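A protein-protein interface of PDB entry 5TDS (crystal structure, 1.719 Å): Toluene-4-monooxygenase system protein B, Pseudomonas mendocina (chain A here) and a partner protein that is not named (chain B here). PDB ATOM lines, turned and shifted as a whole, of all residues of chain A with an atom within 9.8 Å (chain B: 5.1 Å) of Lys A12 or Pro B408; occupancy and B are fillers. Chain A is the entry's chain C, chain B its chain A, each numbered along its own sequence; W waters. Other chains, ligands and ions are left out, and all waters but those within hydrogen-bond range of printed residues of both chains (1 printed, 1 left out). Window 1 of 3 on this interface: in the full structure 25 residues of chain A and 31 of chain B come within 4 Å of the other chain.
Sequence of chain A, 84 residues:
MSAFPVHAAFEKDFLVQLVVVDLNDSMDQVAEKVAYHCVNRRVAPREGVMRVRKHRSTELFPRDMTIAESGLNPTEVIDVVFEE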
ATOM      1  N   ALA A   9       5.920  22.998 -20.859  1.00  0.00           N
ATOM      2  CA  ALA A   9       6.867  22.954 -21.962  1.00  0.00           C
ATOM      3  C   ALA A   9       7.974  23.972 -21.705  1.00  0.00           C
ATOM      4  O   ALA A   9       7.705  25.171 -21.574  1.00  0.00           O
ATOM      5  CB  ALA A   9       6.168  23.229 -23.275  1.00  0.00           C
ATOM      6  N   PHE A  10       9.212  23.490 -21.604  1.00  0.00           N
ATOM      7  CA  PHE A  10      10.353  24.348 -21.296  1.00  0.00           C
ATOM      8  C   PHE A  10      11.059  24.795 -22.565  1.00  0.00           C
ATOM      9  O   PHE A  10      11.305  23.983 -23.452  1.00  0.00           O
ATOM     10  CB  PHE A  10      11.350  23.617 -20.389  1.00  0.00           C
ATOM     11  CG  PHE A  10      12.333  24.531 -19.723  1.00  0.00           C
ATOM     12  CD1 PHE A  10      13.527  24.860 -20.343  1.00  0.00           C
ATOM     13  CD2 PHE A  10      12.050  25.085 -18.484  1.00  0.00           C
ATOM     14  CE1 PHE A  10      14.424  25.726 -19.736  1.00  0.00           C
ATOM     15  CE2 PHE A  10      12.947  25.942 -17.871  1.00  0.00           C
ATOM     16  CZ  PHE A  10      14.133  26.262 -18.498  1.00  0.00           C
ATOM     17  N   GLU A  11      11.403  26.080 -22.641  1.00  0.00           N
ATOM     18  CA  GLU A  11      12.027  26.644 -23.838  1.00  0.00           C
ATOM     19  C   GLU A  11      13.244  25.853 -24.320  1.00  0.00           C
ATOM     20  O   GLU A  11      14.178  25.611 -23.560  1.00  0.00           O
ATOM     21  CB  GLU A  11      12.429  28.101 -23.580  1.00  0.00           C
ATOM     22  CG  GLU A  11      12.947  28.825 -24.819  1.00  0.00           C
ATOM     23  CD  GLU A  11      13.153  30.305 -24.577  1.00  0.00           C
ATOM     24  OE1 GLU A  11      12.393  30.880 -23.775  1.00  0.00           O
ATOM     25  OE2 GLU A  11      14.077  30.887 -25.179  1.00  0.00           O
ATOM     26  N   LYS A  12      13.185  25.443 -25.587  1.00  0.00           N
ATOM     27  CA  LYS A  12      14.249  24.726 -26.296  1.00  0.00           C
ATOM     28  C   LYS A  12      14.287  23.227 -26.013  1.00  0.00           C
ATOM     29  O   LYS A  12      15.127  22.509 -26.564  1.00  0.00           O
ATOM     30  CB  LYS A  12      15.611  25.353 -26.000  1.00  0.00           C
ATOM     31  CG  LYS A  12      15.763  26.739 -26.625  1.00  0.00           C
ATOM     32  CD  LYS A  12      17.200  27.223 -26.589  1.00  0.00           C
ATOM     33  CE  LYS A  12      17.369  28.461 -27.468  1.00  0.00           C
ATOM     34  NZ  LYS A  12      18.799  28.766 -27.722  1.00  0.00           N
ATOM     35  N   ASP A  13      13.372  22.749 -25.178  1.00  0.00           N
ATOM     36  CA  ASP A  13      13.231  21.308 -24.949  1.00  0.00           C
ATOM     37  C   ASP A  13      12.385  20.708 -26.072  1.00  0.00           C
ATOM     38  O   ASP A  13      11.875  21.436 -26.917  1.00  0.00           O
ATOM     39  CB  ASP A  13      12.600  21.057 -23.576  1.00  0.00           C
ATOM     40  CG  ASP A  13      12.867  19.665 -23.034  1.00  0.00           C
ATOM     41  OD1 ASP A  13      13.561  18.856 -23.692  1.00  0.00           O
ATOM     42  OD2 ASP A  13      12.365  19.391 -21.921  1.00  0.00           O
ATOM     43  N   PHE A  14      12.217  19.387 -26.084  1.00  0.00           N
ATOM     44  CA  PHE A  14      11.533  18.737 -27.206  1.00  0.00           C
ATOM     45  C   PHE A  14      10.122  18.237 -26.863  1.00  0.00           C
ATOM     46  O   PHE A  14       9.403  17.757 -27.737  1.00  0.00           O
ATOM     47  CB  PHE A  14      12.382  17.567 -27.736  1.00  0.00           C
ATOM     48  CG  PHE A  14      12.208  16.284 -26.962  1.00  0.00           C
ATOM     49  CD1 PHE A  14      12.866  16.089 -25.763  1.00  0.00           C
ATOM     50  CD2 PHE A  14      11.385  15.276 -27.440  1.00  0.00           C
ATOM     51  CE1 PHE A  14      12.700  14.915 -25.044  1.00  0.00           C
ATOM     52  CE2 PHE A  14      11.221  14.100 -26.735  1.00  0.00           C
ATOM     53  CZ  PHE A  14      11.880  13.916 -25.534  1.00  0.00           C
ATOM     54  N   LEU A  15       9.716  18.361 -25.604  1.00  0.00           N
ATOM     55  CA  LEU A  15       8.432  17.809 -25.202  1.00  0.00           C
ATOM     56  C   LEU A  15       7.731  18.632 -24.131  1.00  0.00           C
ATOM     57  O   LEU A  15       8.271  19.621 -23.618  1.00  0.00           O
ATOM     58  CB  LEU A  15       8.600  16.370 -24.697  1.00  0.00           C
ATOM     59  CG  LEU A  15       9.046  16.190 -23.240  1.00  0.00           C
ATOM     60  CD1 LEU A  15       8.996  14.722 -22.860  1.00  0.00           C
ATOM     61  CD2 LEU A  15      10.440  16.758 -22.996  1.00  0.00           C
ATOM     62  N   VAL A  16       6.516  18.201 -23.817  1.00  0.00           N
ATOM     63  CA  VAL A  16       5.759  18.704 -22.679  1.00  0.00           C
ATOM     64  C   VAL A  16       5.791  17.625 -21.606  1.00  0.00           C
ATOM     65  O   VAL A  16       5.589  16.452 -21.910  1.00  0.00           O
ATOM     66  CB  VAL A  16       4.301  19.026 -23.055  1.00  0.00           C
ATOM     67  CG1 VAL A  16       3.596  19.776 -21.911  1.00  0.00           C
ATOM     68  CG2 VAL A  16       4.246  19.819 -24.365  1.00  0.00           C
ATOM     69  N   CYS A  38      14.570  19.605 -16.991  1.00  0.00           N
ATOM     70  CA  CYS A  38      14.941  20.022 -18.348  1.00  0.00           C
ATOM     71  C   CYS A  38      16.367  20.557 -18.456  1.00  0.00           C
ATOM     72  O   CYS A  38      17.155  20.105 -19.285  1.00  0.00           O
ATOM     73  CB  CYS A  38      13.970  21.095 -18.857  1.00  0.00           C
ATOM     74  SG  CYS A  38      12.243  20.618 -18.709  1.00  0.00           S
ATOM     75  N   VAL A  39      16.691  21.540 -17.624  1.00  0.00           N
ATOM     76  CA  VAL A  39      18.002  22.172 -17.693  1.00  0.00           C
ATOM     77  C   VAL A  39      19.107  21.188 -17.307  1.00  0.00           C
ATOM     78  O   VAL A  39      18.995  20.471 -16.313  1.00  0.00           O
ATOM     79  CB  VAL A  39      18.050  23.415 -16.800  1.00  0.00           C
ATOM     80  CG1 VAL A  39      19.444  24.007 -16.805  1.00  0.00           C
ATOM     81  CG2 VAL A  39      17.023  24.427 -17.286  1.00  0.00           C
ATOM     82  N   ARG A  41      19.665  18.514 -18.687  1.00  0.00           N
ATOM     83  CA  ARG A  41      19.253  17.186 -19.135  1.00  0.00           C
ATOM     84  C   ARG A  41      19.151  17.177 -20.651  1.00  0.00           C
ATOM     85  O   ARG A  41      19.773  16.348 -21.320  1.00  0.00           O
ATOM     86  CB  ARG A  41      17.920  16.780 -18.504  1.00  0.00           C
ATOM     87  CG  ARG A  41      18.019  16.568 -16.994  1.00  0.00           C
ATOM     88  CD  ARG A  41      16.680  16.277 -16.329  1.00  0.00           C
ATOM     89  NE  ARG A  41      16.871  16.037 -14.900  1.00  0.00           N
ATOM     90  CZ  ARG A  41      17.136  14.846 -14.376  1.00  0.00           C
ATOM     91  NH1 ARG A  41      17.202  13.778 -15.161  1.00  0.00           N
ATOM     92  NH2 ARG A  41      17.320  14.720 -13.067  1.00  0.00           N
ATOM     93  N   ARG A  42      18.383  18.121 -21.190  1.00  0.00           N
ATOM     94  CA  ARG A  42      18.229  18.251 -22.637  1.00  0.00           C
ATOM     95  C   ARG A  42      18.316  19.698 -23.094  1.00  0.00           C
ATOM     96  O   ARG A  42      18.257  19.974 -24.287  1.00  0.00           O
ATOM     97  CB  ARG A  42      16.899  17.644 -23.084  1.00  0.00           C
ATOM     98  CG  ARG A  42      16.783  16.143 -22.810  1.00  0.00           C
ATOM     99  CD  ARG A  42      15.389  15.634 -23.127  1.00  0.00           C
ATOM    100  NE  ARG A  42      14.407  16.435 -22.410  1.00  0.00           N
ATOM    101  CZ  ARG A  42      14.034  16.208 -21.157  1.00  0.00           C
ATOM    102  NH1 ARG A  42      13.156  17.010 -20.578  1.00  0.00           N
ATOM    103  NH2 ARG A  42      14.536  15.176 -20.484  1.00  0.00           N
ATOM    104  N   VAL A  43      18.451  20.616 -22.140  1.00  0.00           N
ATOM    105  CA  VAL A  43      18.508  22.046 -22.423  1.00  0.00           C
ATOM    106  C   VAL A  43      19.731  22.663 -21.756  1.00  0.00           C
ATOM    107  O   VAL A  43      19.989  22.423 -20.582  1.00  0.00           O
ATOM    108  CB  VAL A  43      17.231  22.758 -21.924  1.00  0.00           C
ATOM    109  CG1 VAL A  43      17.361  24.263 -22.051  1.00  0.00           C
ATOM    110  CG2 VAL A  43      16.021  22.252 -22.694  1.00  0.00           C
ATOM    111  N   ALA A  44      20.497  23.442 -22.513  1.00  0.00           N
ATOM    112  CA  ALA A  44      21.679  24.091 -21.959  1.00  0.00           C
ATOM    113  C   ALA A  44      21.295  25.140 -20.919  1.00  0.00           C
ATOM    114  O   ALA A  44      20.334  25.885 -21.109  1.00  0.00           O
ATOM    115  CB  ALA A  44      22.497  24.726 -23.067  1.00  0.00           C
ATOM    116  N   PRO A  45      22.057  25.209 -19.816  1.00  0.00           N
ATOM    117  CA  PRO A  45      21.787  26.230 -18.798  1.00  0.00           C
ATOM    118  C   PRO A  45      22.026  27.638 -19.338  1.00  0.00           C
ATOM    119  O   PRO A  45      22.967  27.849 -20.103  1.00  0.00           O
ATOM    120  CB  PRO A  45      22.777  25.887 -17.679  1.00  0.00           C
ATOM    121  CG  PRO A  45      23.897  25.179 -18.376  1.00  0.00           C
ATOM    122  CD  PRO A  45      23.259  24.414 -19.508  1.00  0.00           C
ATOM    123  N   ARG A  46      21.169  28.575 -18.940  1.00  0.00           N
ATOM    124  CA  ARG A  46      21.222  29.957 -19.401  1.00  0.00           C
ATOM    125  C   ARG A  46      21.156  30.924 -18.240  1.00  0.00           C
ATOM    126  O   ARG A  46      20.588  30.619 -17.195  1.00  0.00           O
ATOM    127  CB  ARG A  46      20.056  30.265 -20.342  1.00  0.00           C
ATOM    128  CG  ARG A  46      20.265  29.938 -21.801  1.00  0.00           C
ATOM    129  CD  ARG A  46      19.098  30.504 -22.593  1.00  0.00           C
ATOM    130  NE  ARG A  46      18.749  31.832 -22.094  1.00  0.00           N
ATOM    131  CZ  ARG A  46      17.847  32.638 -22.646  1.00  0.00           C
ATOM    132  NH1 ARG A  46      17.610  33.826 -22.107  1.00  0.00           N
ATOM    133  NH2 ARG A  46      17.186  32.259 -23.733  1.00  0.00           N
ATOM    134  N   ARG A  53       4.049  31.223 -18.455  1.00  0.00           N
ATOM    135  CA  ARG A  53       2.914  31.753 -19.200  1.00  0.00           C
ATOM    136  C   ARG A  53       1.980  30.617 -19.569  1.00  0.00           C
ATOM    137  O   ARG A  53       2.401  29.459 -19.628  1.00  0.00           O
ATOM    138  CB  ARG A  53       3.383  32.473 -20.460  1.00  0.00           C
ATOM    139  CG  ARG A  53       3.899  31.520 -21.519  1.00  0.00           C
ATOM    140  CD  ARG A  53       4.458  32.269 -22.707  1.00  0.00           C
ATOM    141  NE  ARG A  53       4.824  31.356 -23.783  1.00  0.00           N
ATOM    142  CZ  ARG A  53       5.687  31.654 -24.744  1.00  0.00           C
ATOM    143  NH1 ARG A  53       5.967  30.763 -25.684  1.00  0.00           N
ATOM    144  NH2 ARG A  53       6.274  32.844 -24.756  1.00  0.00           N
ATOM    145  N   ASP A  79       3.962  27.249 -20.536  1.00  0.00           N
ATOM    146  CA  ASP A  79       5.334  27.347 -21.040  1.00  0.00           C
ATOM    147  C   ASP A  79       6.233  27.964 -19.973  1.00  0.00           C
ATOM    148  O   ASP A  79       5.803  28.864 -19.248  1.00  0.00           O
ATOM    149  CB  ASP A  79       5.424  28.212 -22.302  1.00  0.00           C
ATOM    150  CG  ASP A  79       4.592  27.687 -23.451  1.00  0.00           C
ATOM    151  OD1 ASP A  79       4.282  26.481 -23.471  1.00  0.00           O
ATOM    152  OD2 ASP A  79       4.258  28.492 -24.349  1.00  0.00           O
ATOM    153  N   VAL A  80       7.476  27.495 -19.891  1.00  0.00           N
ATOM    154  CA  VAL A  80       8.505  28.156 -19.093  1.00  0.00           C
ATOM    155  C   VAL A  80       9.557  28.702 -20.043  1.00  0.00           C
ATOM    156  O   VAL A  80      10.238  27.944 -20.730  1.00  0.00           O
ATOM    157  CB  VAL A  80       9.154  27.208 -18.066  1.00  0.00           C
ATOM    158  CG1 VAL A  80      10.277  27.915 -17.329  1.00  0.00           C
ATOM    159  CG2 VAL A  80       8.106  26.699 -17.080  1.00  0.00           C
ATOM    160  N   VAL A  81       9.669  30.026 -20.089  1.00  0.00           N
ATOM    161  CA  VAL A  81      10.515  30.707 -21.068  1.00  0.00           C
ATOM    162  C   VAL A  81      11.401  31.760 -20.406  1.00  0.00           C
ATOM    163  O   VAL A  81      11.215  32.088 -19.236  1.00  0.00           O
ATOM    164  CB  VAL A  81       9.665  31.388 -22.159  1.00  0.00           C
ATOM    165  CG1 VAL A  81       8.763  30.372 -22.837  1.00  0.00           C
ATOM    166  CG2 VAL A  81       8.837  32.513 -21.558  1.00  0.00           C
ATOM    167  N   PHE A  82      12.350  32.298 -21.167  1.00  0.00           N
ATOM    168  CA  PHE A  82      13.267  33.311 -20.645  1.00  0.00           C
ATOM    169  C   PHE A  82      12.917  34.720 -21.106  1.00  0.00           C
ATOM    170  O   PHE A  82      12.352  34.909 -22.185  1.00  0.00           O
ATOM    171  CB  PHE A  82      14.706  32.986 -21.047  1.00  0.00           C
ATOM    172  CG  PHE A  82      15.270  31.793 -20.341  1.00  0.00           C
ATOM    173  CD1 PHE A  82      15.028  30.512 -20.814  1.00  0.00           C
ATOM    174  CD2 PHE A  82      16.035  31.946 -19.197  1.00  0.00           C
ATOM    175  CE1 PHE A  82      15.540  29.410 -20.158  1.00  0.00           C
ATOM    176  CE2 PHE A  82      16.552  30.845 -18.537  1.00  0.00           C
ATOM    177  CZ  PHE A  82      16.304  29.578 -19.018  1.00  0.00           C
ATOM    178  N   SER B 330      11.914  13.600 -32.615  1.00  0.00           N
ATOM    179  CA  SER B 330      11.519  13.878 -31.240  1.00  0.00           C
ATOM    180  C   SER B 330      11.049  12.603 -30.558  1.00  0.00           C
ATOM    181  O   SER B 330      11.352  12.360 -29.390  1.00  0.00           O
ATOM    182  CB  SER B 330      10.431  14.955 -31.195  1.00  0.00           C
ATOM    183  OG  SER B 330      10.995  16.242 -31.409  1.00  0.00           O
ATOM    184  N   MET B 333      14.151  10.647 -29.557  1.00  0.00           N
ATOM    185  CA  MET B 333      14.756  11.259 -28.392  1.00  0.00           C
ATOM    186  C   MET B 333      14.022  10.849 -27.118  1.00  0.00           C
ATOM    187  O   MET B 333      14.648  10.579 -26.091  1.00  0.00           O
ATOM    188  CB  MET B 333      14.747  12.778 -28.538  1.00  0.00           C
ATOM    189  CG  MET B 333      15.400  13.503 -27.395  1.00  0.00           C
ATOM    190  SD  MET B 333      15.604  15.246 -27.779  1.00  0.00           S
ATOM    191  CE  MET B 333      16.949  15.159 -28.965  1.00  0.00           C
ATOM    192  N   LYS B 367      21.077  21.975 -35.216  1.00  0.00           N
ATOM    193  CA  LYS B 367      20.612  23.195 -34.533  1.00  0.00           C
ATOM    194  C   LYS B 367      19.296  22.962 -33.788  1.00  0.00           C
ATOM    195  O   LYS B 367      18.829  23.820 -33.032  1.00  0.00           O
ATOM    196  CB  LYS B 367      20.447  24.344 -35.530  1.00  0.00           C
ATOM    197  CG  LYS B 367      19.205  24.242 -36.384  1.00  0.00           C
ATOM    198  CD  LYS B 367      19.005  25.490 -37.260  1.00  0.00           C
ATOM    199  CE  LYS B 367      19.965  25.529 -38.423  1.00  0.00           C
ATOM    200  NZ  LYS B 367      19.496  26.473 -39.482  1.00  0.00           N
ATOM    201  N   ARG B 368      18.710  21.790 -34.014  1.00  0.00           N
ATOM    202  CA  ARG B 368      17.433  21.418 -33.420  1.00  0.00           C
ATOM    203  C   ARG B 368      17.667  20.286 -32.425  1.00  0.00           C
ATOM    204  O   ARG B 368      18.095  20.538 -31.306  1.00  0.00           O
ATOM    205  CB  ARG B 368      16.439  21.020 -34.509  1.00  0.00           C
ATOM    206  CG  ARG B 368      15.993  22.194 -35.353  1.00  0.00           C
ATOM    207  CD  ARG B 368      15.491  21.780 -36.727  1.00  0.00           C
ATOM    208  NE  ARG B 368      15.072  22.963 -37.468  1.00  0.00           N
ATOM    209  CZ  ARG B 368      15.335  23.185 -38.750  1.00  0.00           C
ATOM    210  NH1 ARG B 368      16.009  22.290 -39.465  1.00  0.00           N
ATOM    211  NH2 ARG B 368      14.907  24.305 -39.317  1.00  0.00           N
ATOM    212  N   TRP B 369      17.433  19.044 -32.840  1.00  0.00           N
ATOM    213  CA  TRP B 369      17.631  17.893 -31.946  1.00  0.00           C
ATOM    214  C   TRP B 369      19.072  17.752 -31.456  1.00  0.00           C
ATOM    215  O   TRP B 369      19.320  17.283 -30.343  1.00  0.00           O
ATOM    216  CB  TRP B 369      17.173  16.604 -32.643  1.00  0.00           C
ATOM    217  CG  TRP B 369      15.730  16.709 -32.995  1.00  0.00           C
ATOM    218  CD1 TRP B 369      14.653  16.408 -32.194  1.00  0.00           C
ATOM    219  CD2 TRP B 369      15.192  17.231 -34.212  1.00  0.00           C
ATOM    220  NE1 TRP B 369      13.484  16.690 -32.861  1.00  0.00           N
ATOM    221  CE2 TRP B 369      13.788  17.202 -34.097  1.00  0.00           C
ATOM    222  CE3 TRP B 369      15.764  17.710 -35.396  1.00  0.00           C
ATOM    223  CZ2 TRP B 369      12.950  17.624 -35.126  1.00  0.00           C
ATOM    224  CZ3 TRP B 369      14.929  18.131 -36.414  1.00  0.00           C
ATOM    225  CH2 TRP B 369      13.538  18.085 -36.273  1.00  0.00           C
ATOM    226  N   CYS B 372      19.881  19.107 -27.938  1.00  0.00           N
ATOM    227  CA  CYS B 372      19.541  18.215 -26.834  1.00  0.00           C
ATOM    228  C   CYS B 372      20.577  17.102 -26.698  1.00  0.00           C
ATOM    229  O   CYS B 372      21.014  16.772 -25.594  1.00  0.00           O
ATOM    230  CB  CYS B 372      18.148  17.607 -27.038  1.00  0.00           C
ATOM    231  SG  CYS B 372      16.793  18.806 -27.183  1.00  0.00           S
ATOM    232  N   GLY B 406       7.600  18.474 -29.815  1.00  0.00           N
ATOM    233  CA  GLY B 406       7.770  19.485 -30.840  1.00  0.00           C
ATOM    234  C   GLY B 406       9.215  19.538 -31.298  1.00  0.00           C
ATOM    235  O   GLY B 406       9.970  18.578 -31.127  1.00  0.00           O
ATOM    236  N   VAL B 407       9.599  20.667 -31.886  1.00  0.00           N
ATOM    237  CA  VAL B 407      10.965  20.878 -32.347  1.00  0.00           C
ATOM    238  C   VAL B 407      11.757  21.610 -31.275  1.00  0.00           C
ATOM    239  O   VAL B 407      11.334  22.666 -30.818  1.00  0.00           O
ATOM    240  CB  VAL B 407      11.010  21.706 -33.643  1.00  0.00           C
ATOM    241  CG1 VAL B 407      12.450  21.826 -34.134  1.00  0.00           C
ATOM    242  CG2 VAL B 407      10.105  21.078 -34.717  1.00  0.00           C
ATOM    243  N   PRO B 408      12.902  21.049 -30.869  1.00  0.00           N
ATOM    244  CA  PRO B 408      13.732  21.636 -29.813  1.00  0.00           C
ATOM    245  C   PRO B 408      14.828  22.538 -30.358  1.00  0.00           C
ATOM    246  O   PRO B 408      14.939  22.714 -31.569  1.00  0.00           O
ATOM    247  CB  PRO B 408      14.346  20.411 -29.144  1.00  0.00           C
ATOM    248  CG  PRO B 408      14.516  19.425 -30.313  1.00  0.00           C
ATOM    249  CD  PRO B 408      13.402  19.726 -31.296  1.00  0.00           C
ATOM    250  N   GLY B 409      15.644  23.075 -29.459  1.00  0.00           N
ATOM    251  CA  GLY B 409      16.831  23.810 -29.846  1.00  0.00           C
ATOM    252  C   GLY B 409      16.550  25.190 -30.406  1.00  0.00           C
ATOM    253  O   GLY B 409      15.669  25.905 -29.920  1.00  0.00           O
ATOM    254  N   ASP B 410      17.307  25.550 -31.442  1.00  0.00           N
ATOM    255  CA  ASP B 410      17.299  26.894 -32.014  1.00  0.00           C
ATOM    256  C   ASP B 410      15.987  27.280 -32.684  1.00  0.00           C
ATOM    257  O   ASP B 410      15.715  28.462 -32.900  1.00  0.00           O
ATOM    258  CB  ASP B 410      18.412  27.034 -33.048  1.00  0.00           C
ATOM    259  CG  ASP B 410      19.800  26.874 -32.459  1.00  0.00           C
ATOM    260  OD1 ASP B 410      19.927  26.767 -31.225  1.00  0.00           O
ATOM    261  OD2 ASP B 410      20.776  26.872 -33.251  1.00  0.00           O
ATOM    262  N   ASP B 411      15.194  26.284 -33.054  1.00  0.00           N
ATOM    263  CA  ASP B 411      13.912  26.539 -33.693  1.00  0.00           C
ATOM    264  C   ASP B 411      12.794  26.056 -32.804  1.00  0.00           C
ATOM    265  O   ASP B 411      11.871  25.390 -33.275  1.00  0.00           O
ATOM    266  CB  ASP B 411      13.825  25.847 -35.057  1.00  0.00           C
ATOM    267  CG  ASP B 411      14.339  26.713 -36.180  1.00  0.00           C
ATOM    268  OD1 ASP B 411      13.695  27.745 -36.472  1.00  0.00           O
ATOM    269  OD2 ASP B 411      15.381  26.362 -36.774  1.00  0.00           O
ATOM    270  N   TRP B 412      12.884  26.374 -31.515  1.00  0.00           N
ATOM    271  CA  TRP B 412      11.961  25.787 -30.555  1.00  0.00           C
ATOM    272  C   TRP B 412      10.538  26.120 -30.936  1.00  0.00           C
ATOM    273  O   TRP B 412      10.168  27.285 -31.078  1.00  0.00           O
ATOM    274  CB  TRP B 412      12.251  26.262 -29.131  1.00  0.00           C
ATOM    275  CG  TRP B 412      11.308  25.663 -28.108  1.00  0.00           C
ATOM    276  CD1 TRP B 412      11.107  24.332 -27.855  1.00  0.00           C
ATOM    277  CD2 TRP B 412      10.453  26.376 -27.204  1.00  0.00           C
ATOM    278  NE1 TRP B 412      10.169  24.172 -26.857  1.00  0.00           N
ATOM    279  CE2 TRP B 412       9.757  25.412 -26.437  1.00  0.00           C
ATOM    280  CE3 TRP B 412      10.207  27.736 -26.969  1.00  0.00           C
ATOM    281  CZ2 TRP B 412       8.839  25.765 -25.453  1.00  0.00           C
ATOM    282  CZ3 TRP B 412       9.287  28.084 -25.989  1.00  0.00           C
ATOM    283  CH2 TRP B 412       8.620  27.104 -25.242  1.00  0.00           C
HETATM  284  O   HOH W   1      17.886  22.240 -26.136  1.00  0.00           O
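The side-chain hydroxyl of Ser B330 lies within hydrogen-bond range of the indole nitrogen of Trp B369, at 2.9 Å. The guanidinium group (NH2) of Arg A46 is in salt-bridge range of the side-chain carboxylate (OE2) of Glu A11. N of Glu A11 sits at hydrogen-bond distance from O of Val A80 (2.9 Å). OE1 of Glu A11 lies within hydrogen-bond range of N of Phe A82 (3.0 Å). OD2 of Asp A13 lies within hydrogen-bond range of SG of Cys A38 (3.4 Å). NH1 of Arg A42 lies within salt-bridge range of OD2 of Asp A13.
The side-chain sulfur (SG) of Cys B372 sits close to the backbone carbonyl oxygen (O) of Arg A42 (3.4 Å). The backbone NH of Gly B406 sits at hydrogen-bond distance from the backbone carbonyl oxygen of Phe A14. The backbone NH (N) of Gly B409 sits at hydrogen-bond distance from the backbone carbonyl oxygen (O) of Lys A12 (3.0 Å). The backbone carbonyl oxygen (O) of Asp A13 lies close to the indole nitrogen (NE1) of Trp B412.
Printed residues of chain B that touch a printed residue of chain A: Ser B330, Met B333, Cys B372, Gly B406, Pro B408, Gly B409 and Trp B412. Hydrophobic or aromatic side chains of chain B within 4 Å of the printed part of chain A: Met B333, Pro B408 and Trp B412. Of the 21 printed residues of chain A, 7 touch a printed residue of chain B. Hydrophobic or aromatic side chains of chain A that line the printed part of chain B: Phe A14 and Val A81. Among the printed residues, no Asp or Glu carboxylate lies within 4 Å of a Lys or Arg side-chain nitrogen of the other chain.
Printed residues of chain B within 4 Å of Phe A14: Ser B330, Met B333, Gly B406 and Pro B408. Of the printed residues of chain B, Arg A42 touches Cys B372. No residue of chain A comes within 4 Å of Trp B369. Of chain A, only Lys A12 (3.4 Å), Asp A13 (3.4 Å) and Phe A14 (3.7 Å) come within 4 Å of Pro B408. Of chain A, only Lys A12 (3.0 Å) comes within 4 Å of Gly B409. The nearest residue of chain B that does not touch Lys A12 is Cys B372 (4.1 Å).
Water W1 lies within hydrogen-bond range of O of Lys A12, O of Arg A42 and SG of Cys B372.
Phe A10 touches Trp B412 (O to NE1, 3.6 Å). Glu A11 touches Trp B412 (CG to CE3, 3.6 Å). Pro B408 touches Lys A12 (CB to O, 3.4 Å). Lys A12 touches Trp B412 (N to CG, 3.2 Å). CA of Pro B408 touches O of Asp A13 (3.4 Å). Ser B330 touches Phe A14. SD of Met B333 touches CD1 of Phe A14 (3.5 Å). Pro B408 touches Phe A14 (CB to CB, 3.7 Å). CG1 of Val A81 touches CZ3 of Trp B412, 3.9 Å away.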
